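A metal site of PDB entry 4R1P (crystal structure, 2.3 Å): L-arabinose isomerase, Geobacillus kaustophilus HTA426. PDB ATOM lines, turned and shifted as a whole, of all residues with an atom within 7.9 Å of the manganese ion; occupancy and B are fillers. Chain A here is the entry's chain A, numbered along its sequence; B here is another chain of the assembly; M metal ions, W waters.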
ATOM      1  N   MET A 186      19.528  25.649  -0.480  1.00  0.00           N
ATOM      2  CA  MET A 186      19.431  24.750  -1.617  1.00  0.00           C
ATOM      3  C   MET A 186      19.264  23.335  -1.063  1.00  0.00           C
ATOM      4  O   MET A 186      19.981  22.930  -0.142  1.00  0.00           O
ATOM      5  CB  MET A 186      20.691  24.853  -2.463  1.00  0.00           C
ATOM      6  CG  MET A 186      20.715  23.908  -3.637  1.00  0.00           C
ATOM      7  SD  MET A 186      22.157  24.209  -4.692  1.00  0.00           S
ATOM      8  CE  MET A 186      22.116  22.688  -5.648  1.00  0.00           C
ATOM      9  N   THR A 192      26.095  24.714   3.793  1.00  0.00           N
ATOM     10  CA  THR A 192      25.380  25.956   4.021  1.00  0.00           C
ATOM     11  C   THR A 192      24.341  25.803   5.120  1.00  0.00           C
ATOM     12  O   THR A 192      23.702  26.757   5.520  1.00  0.00           O
ATOM     13  CB  THR A 192      24.692  26.430   2.745  1.00  0.00           C
ATOM     14  OG1 THR A 192      23.647  25.516   2.414  1.00  0.00           O
ATOM     15  CG2 THR A 192      25.722  26.526   1.588  1.00  0.00           C
ATOM     16  N   PHE A 280      17.795  30.084  -5.748  1.00  0.00           N
ATOM     17  CA  PHE A 280      17.225  29.933  -7.079  1.00  0.00           C
ATOM     18  C   PHE A 280      16.104  28.890  -7.092  1.00  0.00           C
ATOM     19  O   PHE A 280      15.373  28.801  -8.060  1.00  0.00           O
ATOM     20  CB  PHE A 280      18.318  29.594  -8.118  1.00  0.00           C
ATOM     21  CG  PHE A 280      18.917  28.232  -7.936  1.00  0.00           C
ATOM     22  CD1 PHE A 280      18.273  27.097  -8.425  1.00  0.00           C
ATOM     23  CD2 PHE A 280      20.137  28.083  -7.318  1.00  0.00           C
ATOM     24  CE1 PHE A 280      18.827  25.848  -8.267  1.00  0.00           C
ATOM     25  CE2 PHE A 280      20.697  26.826  -7.157  1.00  0.00           C
ATOM     26  CZ  PHE A 280      20.041  25.702  -7.630  1.00  0.00           C
ATOM     27  N   PHE A 304      25.868  39.131   1.535  1.00  0.00           N
ATOM     28  CA  PHE A 304      25.031  38.295   0.694  1.00  0.00           C
ATOM     29  C   PHE A 304      25.576  36.860   0.667  1.00  0.00           C
ATOM     30  O   PHE A 304      26.792  36.654   0.620  1.00  0.00           O
ATOM     31  CB  PHE A 304      24.945  38.831  -0.744  1.00  0.00           C
ATOM     32  CG  PHE A 304      24.303  37.862  -1.710  1.00  0.00           C
ATOM     33  CD1 PHE A 304      22.923  37.750  -1.780  1.00  0.00           C
ATOM     34  CD2 PHE A 304      25.078  37.033  -2.513  1.00  0.00           C
ATOM     35  CE1 PHE A 304      22.318  36.843  -2.659  1.00  0.00           C
ATOM     36  CE2 PHE A 304      24.480  36.112  -3.377  1.00  0.00           C
ATOM     37  CZ  PHE A 304      23.108  36.026  -3.459  1.00  0.00           C
ATOM     38  N   GLY A 305      24.679  35.885   0.686  1.00  0.00           N
ATOM     39  CA  GLY A 305      25.062  34.514   0.433  1.00  0.00           C
ATOM     40  C   GLY A 305      24.076  33.839  -0.486  1.00  0.00           C
ATOM     41  O   GLY A 305      22.868  33.911  -0.274  1.00  0.00           O
ATOM     42  N   GLY A 306      24.586  33.196  -1.539  1.00  0.00           N
ATOM     43  CA  GLY A 306      23.739  32.441  -2.452  1.00  0.00           C
ATOM     44  C   GLY A 306      23.147  31.200  -1.814  1.00  0.00           C
ATOM     45  O   GLY A 306      23.683  30.696  -0.819  1.00  0.00           O
ATOM     46  N   GLU A 307      22.043  30.716  -2.379  1.00  0.00           N
ATOM     47  CA  GLU A 307      21.451  29.428  -2.011  1.00  0.00           C
ATOM     48  C   GLU A 307      21.117  29.334  -0.535  1.00  0.00           C
ATOM     49  O   GLU A 307      21.246  28.267   0.069  1.00  0.00           O
ATOM     50  CB  GLU A 307      22.369  28.264  -2.397  1.00  0.00           C
ATOM     51  CG  GLU A 307      22.418  27.972  -3.881  1.00  0.00           C
ATOM     52  CD  GLU A 307      23.623  28.609  -4.560  1.00  0.00           C
ATOM     53  OE1 GLU A 307      24.669  28.782  -3.896  1.00  0.00           O
ATOM     54  OE2 GLU A 307      23.517  28.946  -5.755  1.00  0.00           O
ATOM     55  N   ASP A 309      22.671  30.704   1.973  1.00  0.00           N
ATOM     56  CA  ASP A 309      23.871  30.606   2.810  1.00  0.00           C
ATOM     57  C   ASP A 309      24.074  31.796   3.751  1.00  0.00           C
ATOM     58  O   ASP A 309      24.829  32.746   3.443  1.00  0.00           O
ATOM     59  CB  ASP A 309      25.107  30.401   1.946  1.00  0.00           C
ATOM     60  CG  ASP A 309      26.362  30.160   2.752  1.00  0.00           C
ATOM     61  OD1 ASP A 309      26.252  29.987   3.996  1.00  0.00           O
ATOM     62  OD2 ASP A 309      27.451  30.130   2.128  1.00  0.00           O
ATOM     63  N   PHE A 330      31.219  38.300  -1.793  1.00  0.00           N
ATOM     64  CA  PHE A 330      30.850  36.899  -1.833  1.00  0.00           C
ATOM     65  C   PHE A 330      31.608  36.246  -2.994  1.00  0.00           C
ATOM     66  O   PHE A 330      31.799  36.870  -4.033  1.00  0.00           O
ATOM     67  CB  PHE A 330      29.332  36.804  -2.060  1.00  0.00           C
ATOM     68  CG  PHE A 330      28.817  35.391  -2.222  1.00  0.00           C
ATOM     69  CD1 PHE A 330      28.230  34.999  -3.420  1.00  0.00           C
ATOM     70  CD2 PHE A 330      28.882  34.473  -1.174  1.00  0.00           C
ATOM     71  CE1 PHE A 330      27.726  33.699  -3.577  1.00  0.00           C
ATOM     72  CE2 PHE A 330      28.394  33.186  -1.327  1.00  0.00           C
ATOM     73  CZ  PHE A 330      27.807  32.794  -2.525  1.00  0.00           C
ATOM     74  N   MET A 331      32.036  35.006  -2.816  1.00  0.00           N
ATOM     75  CA  MET A 331      32.855  34.338  -3.836  1.00  0.00           C
ATOM     76  C   MET A 331      32.639  32.816  -3.835  1.00  0.00           C
ATOM     77  O   MET A 331      32.281  32.245  -2.819  1.00  0.00           O
ATOM     78  CB  MET A 331      34.336  34.661  -3.619  1.00  0.00           C
ATOM     79  CG  MET A 331      35.302  34.125  -4.666  1.00  0.00           C
ATOM     80  SD  MET A 331      34.869  34.699  -6.323  1.00  0.00           S
ATOM     81  CE  MET A 331      34.841  36.467  -6.063  1.00  0.00           C
ATOM     82  N   GLU A 332      32.859  32.183  -4.966  1.00  0.00           N
ATOM     83  CA  GLU A 332      32.820  30.731  -5.036  1.00  0.00           C
ATOM     84  C   GLU A 332      33.876  30.245  -6.019  1.00  0.00           C
ATOM     85  O   GLU A 332      33.971  30.762  -7.125  1.00  0.00           O
ATOM     86  CB  GLU A 332      31.412  30.250  -5.447  1.00  0.00           C
ATOM     87  CG  GLU A 332      31.272  28.738  -5.615  1.00  0.00           C
ATOM     88  CD  GLU A 332      29.827  28.247  -5.801  1.00  0.00           C
ATOM     89  OE1 GLU A 332      28.871  28.974  -5.437  1.00  0.00           O
ATOM     90  OE2 GLU A 332      29.636  27.114  -6.310  1.00  0.00           O
ATOM     91  N   ASP A 333      34.686  29.264  -5.619  1.00  0.00           N
ATOM     92  CA  ASP A 333      35.672  28.669  -6.531  1.00  0.00           C
ATOM     93  C   ASP A 333      34.915  27.982  -7.649  1.00  0.00           C
ATOM     94  O   ASP A 333      34.031  27.176  -7.399  1.00  0.00           O
ATOM     95  CB  ASP A 333      36.530  27.616  -5.823  1.00  0.00           C
ATOM     96  CG  ASP A 333      37.060  28.093  -4.477  1.00  0.00           C
ATOM     97  OD1 ASP A 333      36.236  28.297  -3.539  1.00  0.00           O
ATOM     98  OD2 ASP A 333      38.299  28.236  -4.343  1.00  0.00           O
ATOM     99  N   TYR A 334      35.262  28.281  -8.900  1.00  0.00           N
ATOM    100  CA  TYR A 334      34.509  27.683 -10.000  1.00  0.00           C
ATOM    101  C   TYR A 334      35.290  26.645 -10.786  1.00  0.00           C
ATOM    102  O   TYR A 334      34.863  25.503 -10.912  1.00  0.00           O
ATOM    103  CB  TYR A 334      33.881  28.754 -10.901  1.00  0.00           C
ATOM    104  CG  TYR A 334      32.370  28.713 -10.855  1.00  0.00           C
ATOM    105  CD1 TYR A 334      31.658  27.895 -11.743  1.00  0.00           C
ATOM    106  CD2 TYR A 334      31.649  29.441  -9.920  1.00  0.00           C
ATOM    107  CE1 TYR A 334      30.277  27.838 -11.706  1.00  0.00           C
ATOM    108  CE2 TYR A 334      30.257  29.380  -9.875  1.00  0.00           C
ATOM    109  CZ  TYR A 334      29.580  28.569 -10.774  1.00  0.00           C
ATOM    110  OH  TYR A 334      28.203  28.495 -10.753  1.00  0.00           O
ATOM    111  N   ALA A 348      33.914  32.921  -9.124  1.00  0.00           N
ATOM    112  CA  ALA A 348      32.748  33.605  -9.667  1.00  0.00           C
ATOM    113  C   ALA A 348      31.488  33.151  -8.921  1.00  0.00           C
ATOM    114  O   ALA A 348      31.556  32.411  -7.946  1.00  0.00           O
ATOM    115  CB  ALA A 348      32.623  33.329 -11.190  1.00  0.00           C
ATOM    116  N   HIS A 349      30.335  33.628  -9.359  1.00  0.00           N
ATOM    117  CA  HIS A 349      29.077  33.006  -8.990  1.00  0.00           C
ATOM    118  C   HIS A 349      28.166  33.112 -10.212  1.00  0.00           C
ATOM    119  O   HIS A 349      28.485  33.842 -11.152  1.00  0.00           O
ATOM    120  CB  HIS A 349      28.434  33.641  -7.755  1.00  0.00           C
ATOM    121  CG  HIS A 349      27.559  32.693  -6.986  1.00  0.00           C
ATOM    122  ND1 HIS A 349      26.188  32.802  -6.941  1.00  0.00           N
ATOM    123  CD2 HIS A 349      27.876  31.597  -6.239  1.00  0.00           C
ATOM    124  CE1 HIS A 349      25.691  31.825  -6.200  1.00  0.00           C
ATOM    125  NE2 HIS A 349      26.692  31.084  -5.767  1.00  0.00           N
ATOM    126  N   MET A 350      27.059  32.377 -10.221  1.00  0.00           N
ATOM    127  CA  MET A 350      26.221  32.351 -11.417  1.00  0.00           C
ATOM    128  C   MET A 350      25.780  33.751 -11.842  1.00  0.00           C
ATOM    129  O   MET A 350      25.575  33.998 -13.023  1.00  0.00           O
ATOM    130  CB  MET A 350      25.030  31.398 -11.245  1.00  0.00           C
ATOM    131  CG  MET A 350      24.004  31.875 -10.240  1.00  0.00           C
ATOM    132  SD  MET A 350      22.813  30.578  -9.869  1.00  0.00           S
ATOM    133  CE  MET A 350      22.308  31.096  -8.215  1.00  0.00           C
ATOM    134  N   GLU A 352      26.299  36.659  -8.999  1.00  0.00           N
ATOM    135  CA  GLU A 352      26.465  37.632  -7.926  1.00  0.00           C
ATOM    136  C   GLU A 352      27.901  37.825  -7.413  1.00  0.00           C
ATOM    137  O   GLU A 352      28.302  37.228  -6.415  1.00  0.00           O
ATOM    138  CB  GLU A 352      25.531  37.297  -6.759  1.00  0.00           C
ATOM    139  CG  GLU A 352      24.113  36.862  -7.170  1.00  0.00           C
ATOM    140  CD  GLU A 352      23.963  35.349  -7.353  1.00  0.00           C
ATOM    141  OE1 GLU A 352      24.842  34.739  -7.988  1.00  0.00           O
ATOM    142  OE2 GLU A 352      22.978  34.771  -6.845  1.00  0.00           O
ATOM    143  N   HIS A 447      32.608  25.924  -0.121  1.00  0.00           N
ATOM    144  CA  HIS A 447      32.821  26.390  -1.489  1.00  0.00           C
ATOM    145  C   HIS A 447      32.466  27.889  -1.634  1.00  0.00           C
ATOM    146  O   HIS A 447      32.892  28.566  -2.571  1.00  0.00           O
ATOM    147  CB  HIS A 447      32.007  25.528  -2.467  1.00  0.00           C
ATOM    148  CG  HIS A 447      30.528  25.581  -2.246  1.00  0.00           C
ATOM    149  ND1 HIS A 447      29.932  25.207  -1.066  1.00  0.00           N
ATOM    150  CD2 HIS A 447      29.515  25.976  -3.062  1.00  0.00           C
ATOM    151  CE1 HIS A 447      28.623  25.354  -1.157  1.00  0.00           C
ATOM    152  NE2 HIS A 447      28.346  25.826  -2.359  1.00  0.00           N
ATOM    153  N   HIS A 448      31.656  28.386  -0.699  1.00  0.00           N
ATOM    154  CA  HIS A 448      31.332  29.806  -0.617  1.00  0.00           C
ATOM    155  C   HIS A 448      32.268  30.447   0.367  1.00  0.00           C
ATOM    156  O   HIS A 448      32.538  29.892   1.410  1.00  0.00           O
ATOM    157  CB  HIS A 448      29.921  29.968  -0.061  1.00  0.00           C
ATOM    158  CG  HIS A 448      28.859  29.650  -1.046  1.00  0.00           C
ATOM    159  ND1 HIS A 448      27.518  29.635  -0.725  1.00  0.00           N
ATOM    160  CD2 HIS A 448      28.928  29.323  -2.367  1.00  0.00           C
ATOM    161  CE1 HIS A 448      26.812  29.328  -1.796  1.00  0.00           C
ATOM    162  NE2 HIS A 448      27.647  29.144  -2.798  1.00  0.00           N
ATOM    163  N   PHE B  84      29.176  20.009  -8.743  1.00  0.00           N
ATOM    164  CA  PHE B  84      28.534  20.139  -7.453  1.00  0.00           C
ATOM    165  C   PHE B  84      27.658  18.923  -7.236  1.00  0.00           C
ATOM    166  O   PHE B  84      26.946  18.500  -8.139  1.00  0.00           O
ATOM    167  CB  PHE B  84      27.675  21.391  -7.393  1.00  0.00           C
ATOM    168  CG  PHE B  84      27.337  21.829  -6.000  1.00  0.00           C
ATOM    169  CD1 PHE B  84      28.351  22.075  -5.072  1.00  0.00           C
ATOM    170  CD2 PHE B  84      26.016  22.020  -5.622  1.00  0.00           C
ATOM    171  CE1 PHE B  84      28.047  22.495  -3.782  1.00  0.00           C
ATOM    172  CE2 PHE B  84      25.697  22.427  -4.336  1.00  0.00           C
ATOM    173  CZ  PHE B  84      26.719  22.664  -3.413  1.00  0.00           C
ATOM    174  N   HIS B 129      34.493  23.609  -6.718  1.00  0.00           N
ATOM    175  CA  HIS B 129      33.616  23.761  -5.564  1.00  0.00           C
ATOM    176  C   HIS B 129      32.878  22.508  -5.112  1.00  0.00           C
ATOM    177  O   HIS B 129      32.547  22.370  -3.938  1.00  0.00           O
ATOM    178  CB  HIS B 129      32.686  24.989  -5.695  1.00  0.00           C
ATOM    179  CG  HIS B 129      31.717  24.949  -6.826  1.00  0.00           C
ATOM    180  ND1 HIS B 129      31.887  25.693  -7.978  1.00  0.00           N
ATOM    181  CD2 HIS B 129      30.532  24.312  -6.964  1.00  0.00           C
ATOM    182  CE1 HIS B 129      30.859  25.500  -8.782  1.00  0.00           C
ATOM    183  NE2 HIS B 129      30.023  24.662  -8.190  1.00  0.00           N
HETATM  184 MN    MN M   1      26.818  28.828  -4.839  1.00  0.00          MN
HETATM  185  O   HOH W   1      26.779  26.529  -5.051  1.00  0.00           O
HETATM  186  O   HOH W   2      26.370  27.269  -7.102  1.00  0.00           O
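O of Glu 332 sits at hydrogen-bond distance from N of Ala 348. OE2 of Glu 332 sits close to NE2 of His 129 of chain B. A ring nitrogen (NE2) of His 447 lies close to a ring nitrogen (NE2) of His 448 (3.4 Å). The backbone carbonyl oxygen (O) of Glu 307 lies within hydrogen-bond range of the backbone NH (N) of Met 186. The side-chain carboxylate (OE1) of Glu 352 lies within hydrogen-bond range of a ring nitrogen (ND1) of His 349. A ring nitrogen (ND1) of His 448 lies within hydrogen-bond range of the side-chain carboxylate of Asp 309, at 2.9 Å.
The nearest printed residue that does not touch the manganese ion is His 447 (4.2 Å).
The manganese ion is bound by the side-chain carboxylate (OE1) of Glu 332 (2.1 Å), a ring nitrogen (NE2) of His 448 (2.2 Å), water W1 (2.3 Å), the side-chain carboxylate (OE1) of Glu 307 (2.3 Å) and a ring nitrogen (NE2) of His 349 (2.4 Å). Slightly farther from the manganese ion lies water W2 (2.8 Å).
Water W1 lies within hydrogen-bond range of OE2 of Glu 332 (3.2 Å) and NE2 of His 447 (3.2 Å).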
